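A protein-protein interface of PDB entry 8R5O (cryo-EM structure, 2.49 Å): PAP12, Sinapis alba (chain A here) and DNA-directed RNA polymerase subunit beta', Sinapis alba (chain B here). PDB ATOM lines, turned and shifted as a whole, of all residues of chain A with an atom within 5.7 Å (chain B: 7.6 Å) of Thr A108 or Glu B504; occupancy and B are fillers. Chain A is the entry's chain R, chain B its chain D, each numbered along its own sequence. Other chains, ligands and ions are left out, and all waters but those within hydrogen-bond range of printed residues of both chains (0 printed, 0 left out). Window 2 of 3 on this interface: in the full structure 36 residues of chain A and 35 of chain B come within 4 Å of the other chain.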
ATOM      1  N   VAL A 100      -5.313  14.081 -15.331  1.00  0.00           N
ATOM      2  CA  VAL A 100      -5.378  15.537 -15.423  1.00  0.00           C
ATOM      3  C   VAL A 100      -4.364  16.053 -16.437  1.00  0.00           C
ATOM      4  O   VAL A 100      -4.670  16.932 -17.250  1.00  0.00           O
ATOM      5  CB  VAL A 100      -5.169  16.171 -14.035  1.00  0.00           C
ATOM      6  CG1 VAL A 100      -5.078  17.682 -14.145  1.00  0.00           C
ATOM      7  CG2 VAL A 100      -6.296  15.775 -13.098  1.00  0.00           C
ATOM      8  N   VAL A 103      -5.535  15.211 -20.062  1.00  0.00           N
ATOM      9  CA  VAL A 103      -6.618  16.087 -20.504  1.00  0.00           C
ATOM     10  C   VAL A 103      -6.076  17.459 -20.880  1.00  0.00           C
ATOM     11  O   VAL A 103      -6.462  18.037 -21.902  1.00  0.00           O
ATOM     12  CB  VAL A 103      -7.708  16.183 -19.419  1.00  0.00           C
ATOM     13  CG1 VAL A 103      -8.675  17.313 -19.726  1.00  0.00           C
ATOM     14  CG2 VAL A 103      -8.456  14.866 -19.300  1.00  0.00           C
ATOM     15  N   ALA A 104      -5.172  18.003 -20.062  1.00  0.00           N
ATOM     16  CA  ALA A 104      -4.578  19.300 -20.370  1.00  0.00           C
ATOM     17  C   ALA A 104      -3.745  19.239 -21.644  1.00  0.00           C
ATOM     18  O   ALA A 104      -3.754  20.180 -22.445  1.00  0.00           O
ATOM     19  CB  ALA A 104      -3.726  19.782 -19.197  1.00  0.00           C
ATOM     20  N   ALA A 105      -3.008  18.144 -21.842  1.00  0.00           N
ATOM     21  CA  ALA A 105      -2.227  17.991 -23.066  1.00  0.00           C
ATOM     22  C   ALA A 105      -3.130  17.938 -24.292  1.00  0.00           C
ATOM     23  O   ALA A 105      -2.832  18.560 -25.318  1.00  0.00           O
ATOM     24  CB  ALA A 105      -1.358  16.738 -22.982  1.00  0.00           C
ATOM     25  N   GLU A 106      -4.238  17.200 -24.206  1.00  0.00           N
ATOM     26  CA  GLU A 106      -5.179  17.150 -25.320  1.00  0.00           C
ATOM     27  C   GLU A 106      -5.870  18.492 -25.531  1.00  0.00           C
ATOM     28  O   GLU A 106      -6.148  18.870 -26.673  1.00  0.00           O
ATOM     29  CB  GLU A 106      -6.210  16.047 -25.087  1.00  0.00           C
ATOM     30  CG  GLU A 106      -7.152  15.816 -26.256  1.00  0.00           C
ATOM     31  CD  GLU A 106      -8.029  14.594 -26.069  1.00  0.00           C
ATOM     32  OE1 GLU A 106      -7.645  13.695 -25.293  1.00  0.00           O
ATOM     33  OE2 GLU A 106      -9.107  14.535 -26.696  1.00  0.00           O
ATOM     34  N   ALA A 107      -6.151  19.222 -24.448  1.00  0.00           N
ATOM     35  CA  ALA A 107      -6.785  20.531 -24.578  1.00  0.00           C
ATOM     36  C   ALA A 107      -5.853  21.532 -25.247  1.00  0.00           C
ATOM     37  O   ALA A 107      -6.302  22.381 -26.026  1.00  0.00           O
ATOM     38  CB  ALA A 107      -7.227  21.040 -23.208  1.00  0.00           C
ATOM     39  N   THR A 108      -4.555  21.457 -24.948  1.00  0.00           N
ATOM     40  CA  THR A 108      -3.591  22.337 -25.603  1.00  0.00           C
ATOM     41  C   THR A 108      -3.563  22.095 -27.106  1.00  0.00           C
ATOM     42  O   THR A 108      -3.453  23.041 -27.893  1.00  0.00           O
ATOM     43  CB  THR A 108      -2.201  22.133 -24.999  1.00  0.00           C
ATOM     44  OG1 THR A 108      -2.247  22.393 -23.592  1.00  0.00           O
ATOM     45  CG2 THR A 108      -1.195  23.070 -25.643  1.00  0.00           C
ATOM     46  N   GLU A 109      -3.673  20.832 -27.524  1.00  0.00           N
ATOM     47  CA  GLU A 109      -3.679  20.517 -28.949  1.00  0.00           C
ATOM     48  C   GLU A 109      -4.891  21.115 -29.651  1.00  0.00           C
ATOM     49  O   GLU A 109      -4.794  21.542 -30.808  1.00  0.00           O
ATOM     50  CB  GLU A 109      -3.638  19.003 -29.148  1.00  0.00           C
ATOM     51  CG  GLU A 109      -2.323  18.364 -28.746  1.00  0.00           C
ATOM     52  CD  GLU A 109      -1.468  17.999 -29.942  1.00  0.00           C
ATOM     53  OE1 GLU A 109      -2.007  17.400 -30.895  1.00  0.00           O
ATOM     54  OE2 GLU A 109      -0.260  18.316 -29.931  1.00  0.00           O
ATOM     55  N   TYR A 110      -6.047  21.142 -28.979  1.00  0.00           N
ATOM     56  CA  TYR A 110      -7.240  21.724 -29.587  1.00  0.00           C
ATOM     57  C   TYR A 110      -7.046  23.206 -29.882  1.00  0.00           C
ATOM     58  O   TYR A 110      -7.432  23.689 -30.952  1.00  0.00           O
ATOM     59  CB  TYR A 110      -8.456  21.537 -28.677  1.00  0.00           C
ATOM     60  CG  TYR A 110      -9.000  20.127 -28.578  1.00  0.00           C
ATOM     61  CD1 TYR A 110      -8.332  19.051 -29.146  1.00  0.00           C
ATOM     62  CD2 TYR A 110     -10.197  19.877 -27.919  1.00  0.00           C
ATOM     63  CE1 TYR A 110      -8.835  17.767 -29.050  1.00  0.00           C
ATOM     64  CE2 TYR A 110     -10.708  18.599 -27.822  1.00  0.00           C
ATOM     65  CZ  TYR A 110     -10.023  17.547 -28.387  1.00  0.00           C
ATOM     66  OH  TYR A 110     -10.531  16.274 -28.290  1.00  0.00           O
ATOM     67  N   VAL A 111      -6.455  23.942 -28.940  1.00  0.00           N
ATOM     68  CA  VAL A 111      -6.329  25.388 -29.092  1.00  0.00           C
ATOM     69  C   VAL A 111      -5.350  25.731 -30.210  1.00  0.00           C
ATOM     70  O   VAL A 111      -5.575  26.672 -30.979  1.00  0.00           O
ATOM     71  CB  VAL A 111      -5.918  26.030 -27.755  1.00  0.00           C
ATOM     72  CG1 VAL A 111      -5.863  27.542 -27.884  1.00  0.00           C
ATOM     73  CG2 VAL A 111      -6.889  25.624 -26.658  1.00  0.00           C
ATOM     74  N   GLU A 112      -4.250  24.982 -30.316  1.00  0.00           N
ATOM     75  CA  GLU A 112      -3.313  25.209 -31.411  1.00  0.00           C
ATOM     76  C   GLU A 112      -3.960  24.915 -32.758  1.00  0.00           C
ATOM     77  O   GLU A 112      -3.743  25.643 -33.734  1.00  0.00           O
ATOM     78  CB  GLU A 112      -2.062  24.351 -31.225  1.00  0.00           C
ATOM     79  CG  GLU A 112      -1.405  24.469 -29.860  1.00  0.00           C
ATOM     80  CD  GLU A 112      -0.656  25.773 -29.668  1.00  0.00           C
ATOM     81  OE1 GLU A 112      -0.488  26.523 -30.652  1.00  0.00           O
ATOM     82  OE2 GLU A 112      -0.230  26.046 -28.525  1.00  0.00           O
ATOM     83  N   LYS A 113      -4.755  23.846 -32.831  1.00  0.00           N
ATOM     84  CA  LYS A 113      -5.393  23.470 -34.088  1.00  0.00           C
ATOM     85  C   LYS A 113      -6.425  24.507 -34.517  1.00  0.00           C
ATOM     86  O   LYS A 113      -6.411  24.973 -35.662  1.00  0.00           O
ATOM     87  CB  LYS A 113      -6.041  22.092 -33.942  1.00  0.00           C
ATOM     88  CG  LYS A 113      -6.238  21.336 -35.244  1.00  0.00           C
ATOM     89  CD  LYS A 113      -7.413  20.374 -35.143  1.00  0.00           C
ATOM     90  CE  LYS A 113      -7.419  19.631 -33.816  1.00  0.00           C
ATOM     91  NZ  LYS A 113      -8.710  18.925 -33.587  1.00  0.00           N
ATOM     92  N   PRO B 500      -7.530  30.670 -12.698  1.00  0.00           N
ATOM     93  CA  PRO B 500      -6.483  29.945 -13.429  1.00  0.00           C
ATOM     94  C   PRO B 500      -6.397  30.420 -14.871  1.00  0.00           C
ATOM     95  O   PRO B 500      -7.412  30.643 -15.533  1.00  0.00           O
ATOM     96  CB  PRO B 500      -6.939  28.483 -13.344  1.00  0.00           C
ATOM     97  CG  PRO B 500      -7.853  28.434 -12.167  1.00  0.00           C
ATOM     98  CD  PRO B 500      -8.539  29.763 -12.130  1.00  0.00           C
ATOM     99  N   LEU B 501      -5.167  30.573 -15.358  1.00  0.00           N
ATOM    100  CA  LEU B 501      -4.930  31.089 -16.702  1.00  0.00           C
ATOM    101  C   LEU B 501      -4.606  29.977 -17.693  1.00  0.00           C
ATOM    102  O   LEU B 501      -5.292  29.826 -18.707  1.00  0.00           O
ATOM    103  CB  LEU B 501      -3.801  32.129 -16.675  1.00  0.00           C
ATOM    104  CG  LEU B 501      -4.033  33.378 -15.822  1.00  0.00           C
ATOM    105  CD1 LEU B 501      -2.842  34.321 -15.911  1.00  0.00           C
ATOM    106  CD2 LEU B 501      -5.313  34.086 -16.235  1.00  0.00           C
ATOM    107  N   SER B 502      -3.571  29.192 -17.414  1.00  0.00           N
ATOM    108  CA  SER B 502      -3.166  28.140 -18.331  1.00  0.00           C
ATOM    109  C   SER B 502      -4.171  26.992 -18.314  1.00  0.00           C
ATOM    110  O   SER B 502      -4.915  26.794 -17.349  1.00  0.00           O
ATOM    111  CB  SER B 502      -1.776  27.622 -17.971  1.00  0.00           C
ATOM    112  OG  SER B 502      -1.789  26.962 -16.718  1.00  0.00           O
ATOM    113  N   LEU B 503      -4.189  26.232 -19.409  1.00  0.00           N
ATOM    114  CA  LEU B 503      -5.067  25.069 -19.485  1.00  0.00           C
ATOM    115  C   LEU B 503      -4.670  24.000 -18.477  1.00  0.00           C
ATOM    116  O   LEU B 503      -5.530  23.254 -17.999  1.00  0.00           O
ATOM    117  CB  LEU B 503      -5.063  24.495 -20.902  1.00  0.00           C
ATOM    118  CG  LEU B 503      -5.711  25.367 -21.977  1.00  0.00           C
ATOM    119  CD1 LEU B 503      -5.498  24.776 -23.358  1.00  0.00           C
ATOM    120  CD2 LEU B 503      -7.193  25.541 -21.691  1.00  0.00           C
ATOM    121  N   GLU B 504      -3.379  23.905 -18.148  1.00  0.00           N
ATOM    122  CA  GLU B 504      -2.950  22.979 -17.106  1.00  0.00           C
ATOM    123  C   GLU B 504      -3.544  23.359 -15.755  1.00  0.00           C
ATOM    124  O   GLU B 504      -3.972  22.489 -14.990  1.00  0.00           O
ATOM    125  CB  GLU B 504      -1.423  22.939 -17.027  1.00  0.00           C
ATOM    126  CG  GLU B 504      -0.729  22.563 -18.328  1.00  0.00           C
ATOM    127  CD  GLU B 504      -0.513  23.754 -19.243  1.00  0.00           C
ATOM    128  OE1 GLU B 504      -0.287  24.868 -18.727  1.00  0.00           O
ATOM    129  OE2 GLU B 504      -0.574  23.577 -20.477  1.00  0.00           O
ATOM    130  N   ALA B 505      -3.575  24.657 -15.445  1.00  0.00           N
ATOM    131  CA  ALA B 505      -4.157  25.104 -14.185  1.00  0.00           C
ATOM    132  C   ALA B 505      -5.674  24.977 -14.186  1.00  0.00           C
ATOM    133  O   ALA B 505      -6.268  24.663 -13.149  1.00  0.00           O
ATOM    134  CB  ALA B 505      -3.743  26.546 -13.897  1.00  0.00           C
ATOM    135  N   GLN B 506      -6.318  25.220 -15.330  1.00  0.00           N
ATOM    136  CA  GLN B 506      -7.767  25.067 -15.407  1.00  0.00           C
ATOM    137  C   GLN B 506      -8.186  23.606 -15.300  1.00  0.00           C
ATOM    138  O   GLN B 506      -9.244  23.309 -14.735  1.00  0.00           O
ATOM    139  CB  GLN B 506      -8.295  25.673 -16.704  1.00  0.00           C
ATOM    140  CG  GLN B 506      -8.054  27.162 -16.851  1.00  0.00           C
ATOM    141  CD  GLN B 506      -8.672  27.726 -18.113  1.00  0.00           C
ATOM    142  OE1 GLN B 506      -9.845  27.487 -18.402  1.00  0.00           O
ATOM    143  NE2 GLN B 506      -7.884  28.469 -18.878  1.00  0.00           N
ATOM    144  N   ALA B 507      -7.385  22.687 -15.842  1.00  0.00           N
ATOM    145  CA  ALA B 507      -7.692  21.268 -15.702  1.00  0.00           C
ATOM    146  C   ALA B 507      -7.610  20.828 -14.247  1.00  0.00           C
ATOM    147  O   ALA B 507      -8.479  20.095 -13.763  1.00  0.00           O
ATOM    148  CB  ALA B 507      -6.747  20.436 -16.569  1.00  0.00           C
ATOM    149  N   GLU B 508      -6.574  21.271 -13.534  1.00  0.00           N
ATOM    150  CA  GLU B 508      -6.420  20.898 -12.134  1.00  0.00           C
ATOM    151  C   GLU B 508      -7.571  21.425 -11.288  1.00  0.00           C
ATOM    152  O   GLU B 508      -8.095  20.711 -10.426  1.00  0.00           O
ATOM    153  CB  GLU B 508      -5.080  21.409 -11.606  1.00  0.00           C
ATOM    154  CG  GLU B 508      -3.877  20.725 -12.229  1.00  0.00           C
ATOM    155  CD  GLU B 508      -2.563  21.355 -11.820  1.00  0.00           C
ATOM    156  OE1 GLU B 508      -2.586  22.418 -11.168  1.00  0.00           O
ATOM    157  OE2 GLU B 508      -1.502  20.786 -12.152  1.00  0.00           O
ATOM    158  N   ALA B 509      -7.989  22.670 -11.531  1.00  0.00           N
ATOM    159  CA  ALA B 509      -9.075  23.254 -10.753  1.00  0.00           C
ATOM    160  C   ALA B 509     -10.376  22.482 -10.941  1.00  0.00           C
ATOM    161  O   ALA B 509     -11.089  22.211  -9.969  1.00  0.00           O
ATOM    162  CB  ALA B 509      -9.261  24.722 -11.137  1.00  0.00           C
ATOM    163  N   ARG B 510     -10.700  22.113 -12.179  1.00  0.00           N
ATOM    164  CA  ARG B 510     -11.970  21.443 -12.435  1.00  0.00           C
ATOM    165  C   ARG B 510     -11.936  19.983 -11.997  1.00  0.00           C
ATOM    166  O   ARG B 510     -12.940  19.455 -11.507  1.00  0.00           O
ATOM    167  CB  ARG B 510     -12.331  21.551 -13.917  1.00  0.00           C
ATOM    168  CG  ARG B 510     -13.674  20.934 -14.270  1.00  0.00           C
ATOM    169  CD  ARG B 510     -14.780  21.517 -13.412  1.00  0.00           C
ATOM    170  NE  ARG B 510     -16.036  20.790 -13.553  1.00  0.00           N
ATOM    171  CZ  ARG B 510     -16.380  19.736 -12.824  1.00  0.00           C
ATOM    172  NH1 ARG B 510     -15.579  19.248 -11.892  1.00  0.00           N
ATOM    173  NH2 ARG B 510     -17.560  19.161 -13.033  1.00  0.00           N
ATOM    174  N   LEU B 512      -9.581  18.310  -9.857  1.00  0.00           N
ATOM    175  CA  LEU B 512      -9.019  17.933  -8.569  1.00  0.00           C
ATOM    176  C   LEU B 512      -9.561  18.732  -7.393  1.00  0.00           C
ATOM    177  O   LEU B 512      -9.654  18.185  -6.293  1.00  0.00           O
ATOM    178  CB  LEU B 512      -7.488  18.071  -8.594  1.00  0.00           C
ATOM    179  CG  LEU B 512      -6.730  17.152  -9.555  1.00  0.00           C
ATOM    180  CD1 LEU B 512      -5.253  17.498  -9.575  1.00  0.00           C
ATOM    181  CD2 LEU B 512      -6.934  15.696  -9.176  1.00  0.00           C
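Glu B508 touches Val A100 (CG to CG1, 3.8 Å).
CG2 of Val A100 touches CG of Leu B512, 3.8 Å away.
Glu B504 touches Ala A104 (CA to CB, 3.9 Å).
Leu B503 touches Ala A107 (CD1 to O, 3.7 Å).
N of Thr A108 touches CD1 of Leu B503, 3.8 Å away.
Glu B504 touches Thr A108 (OE2 to OG1, 3.7 Å).
CG2 of Val A111 touches CD1 of Leu B503 (3.7 Å).
Printed residues of chain B within 4 Å of Val A100: Glu B508 and Leu B512.
Thr A108 touches just these residues of chain B: Leu B503 (3.8 Å) and Glu B504 (3.7 Å).
Printed residues of chain B within 4 Å of Val A111: Leu B503 (3.7 Å).
Ser B502 touches none of the printed residues of chain A.
Glu B504 touches just these residues of chain A: Ala A104 (3.9 Å) and Thr A108 (3.7 Å).
OG1 of Thr A108 sits at hydrogen-bond distance from O of Ala A104 (2.9 Å).
The side-chain hydroxyl (OG) of Ser B502 lies close to the side-chain carboxylate (OE1) of Glu B504 (3.3 Å).
Of the 12 printed residues of chain B, 4 touch a printed residue of chain A.
Along chain B the printed residues that touch a printed residue of chain A span positions 503 to 512.
Of the 12 printed residues of chain A, 5 touch a printed residue of chain B.
Printed residues of chain A that touch a printed residue of chain B: Val A100, Ala A104, Ala A107, Thr A108 and Val A111.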
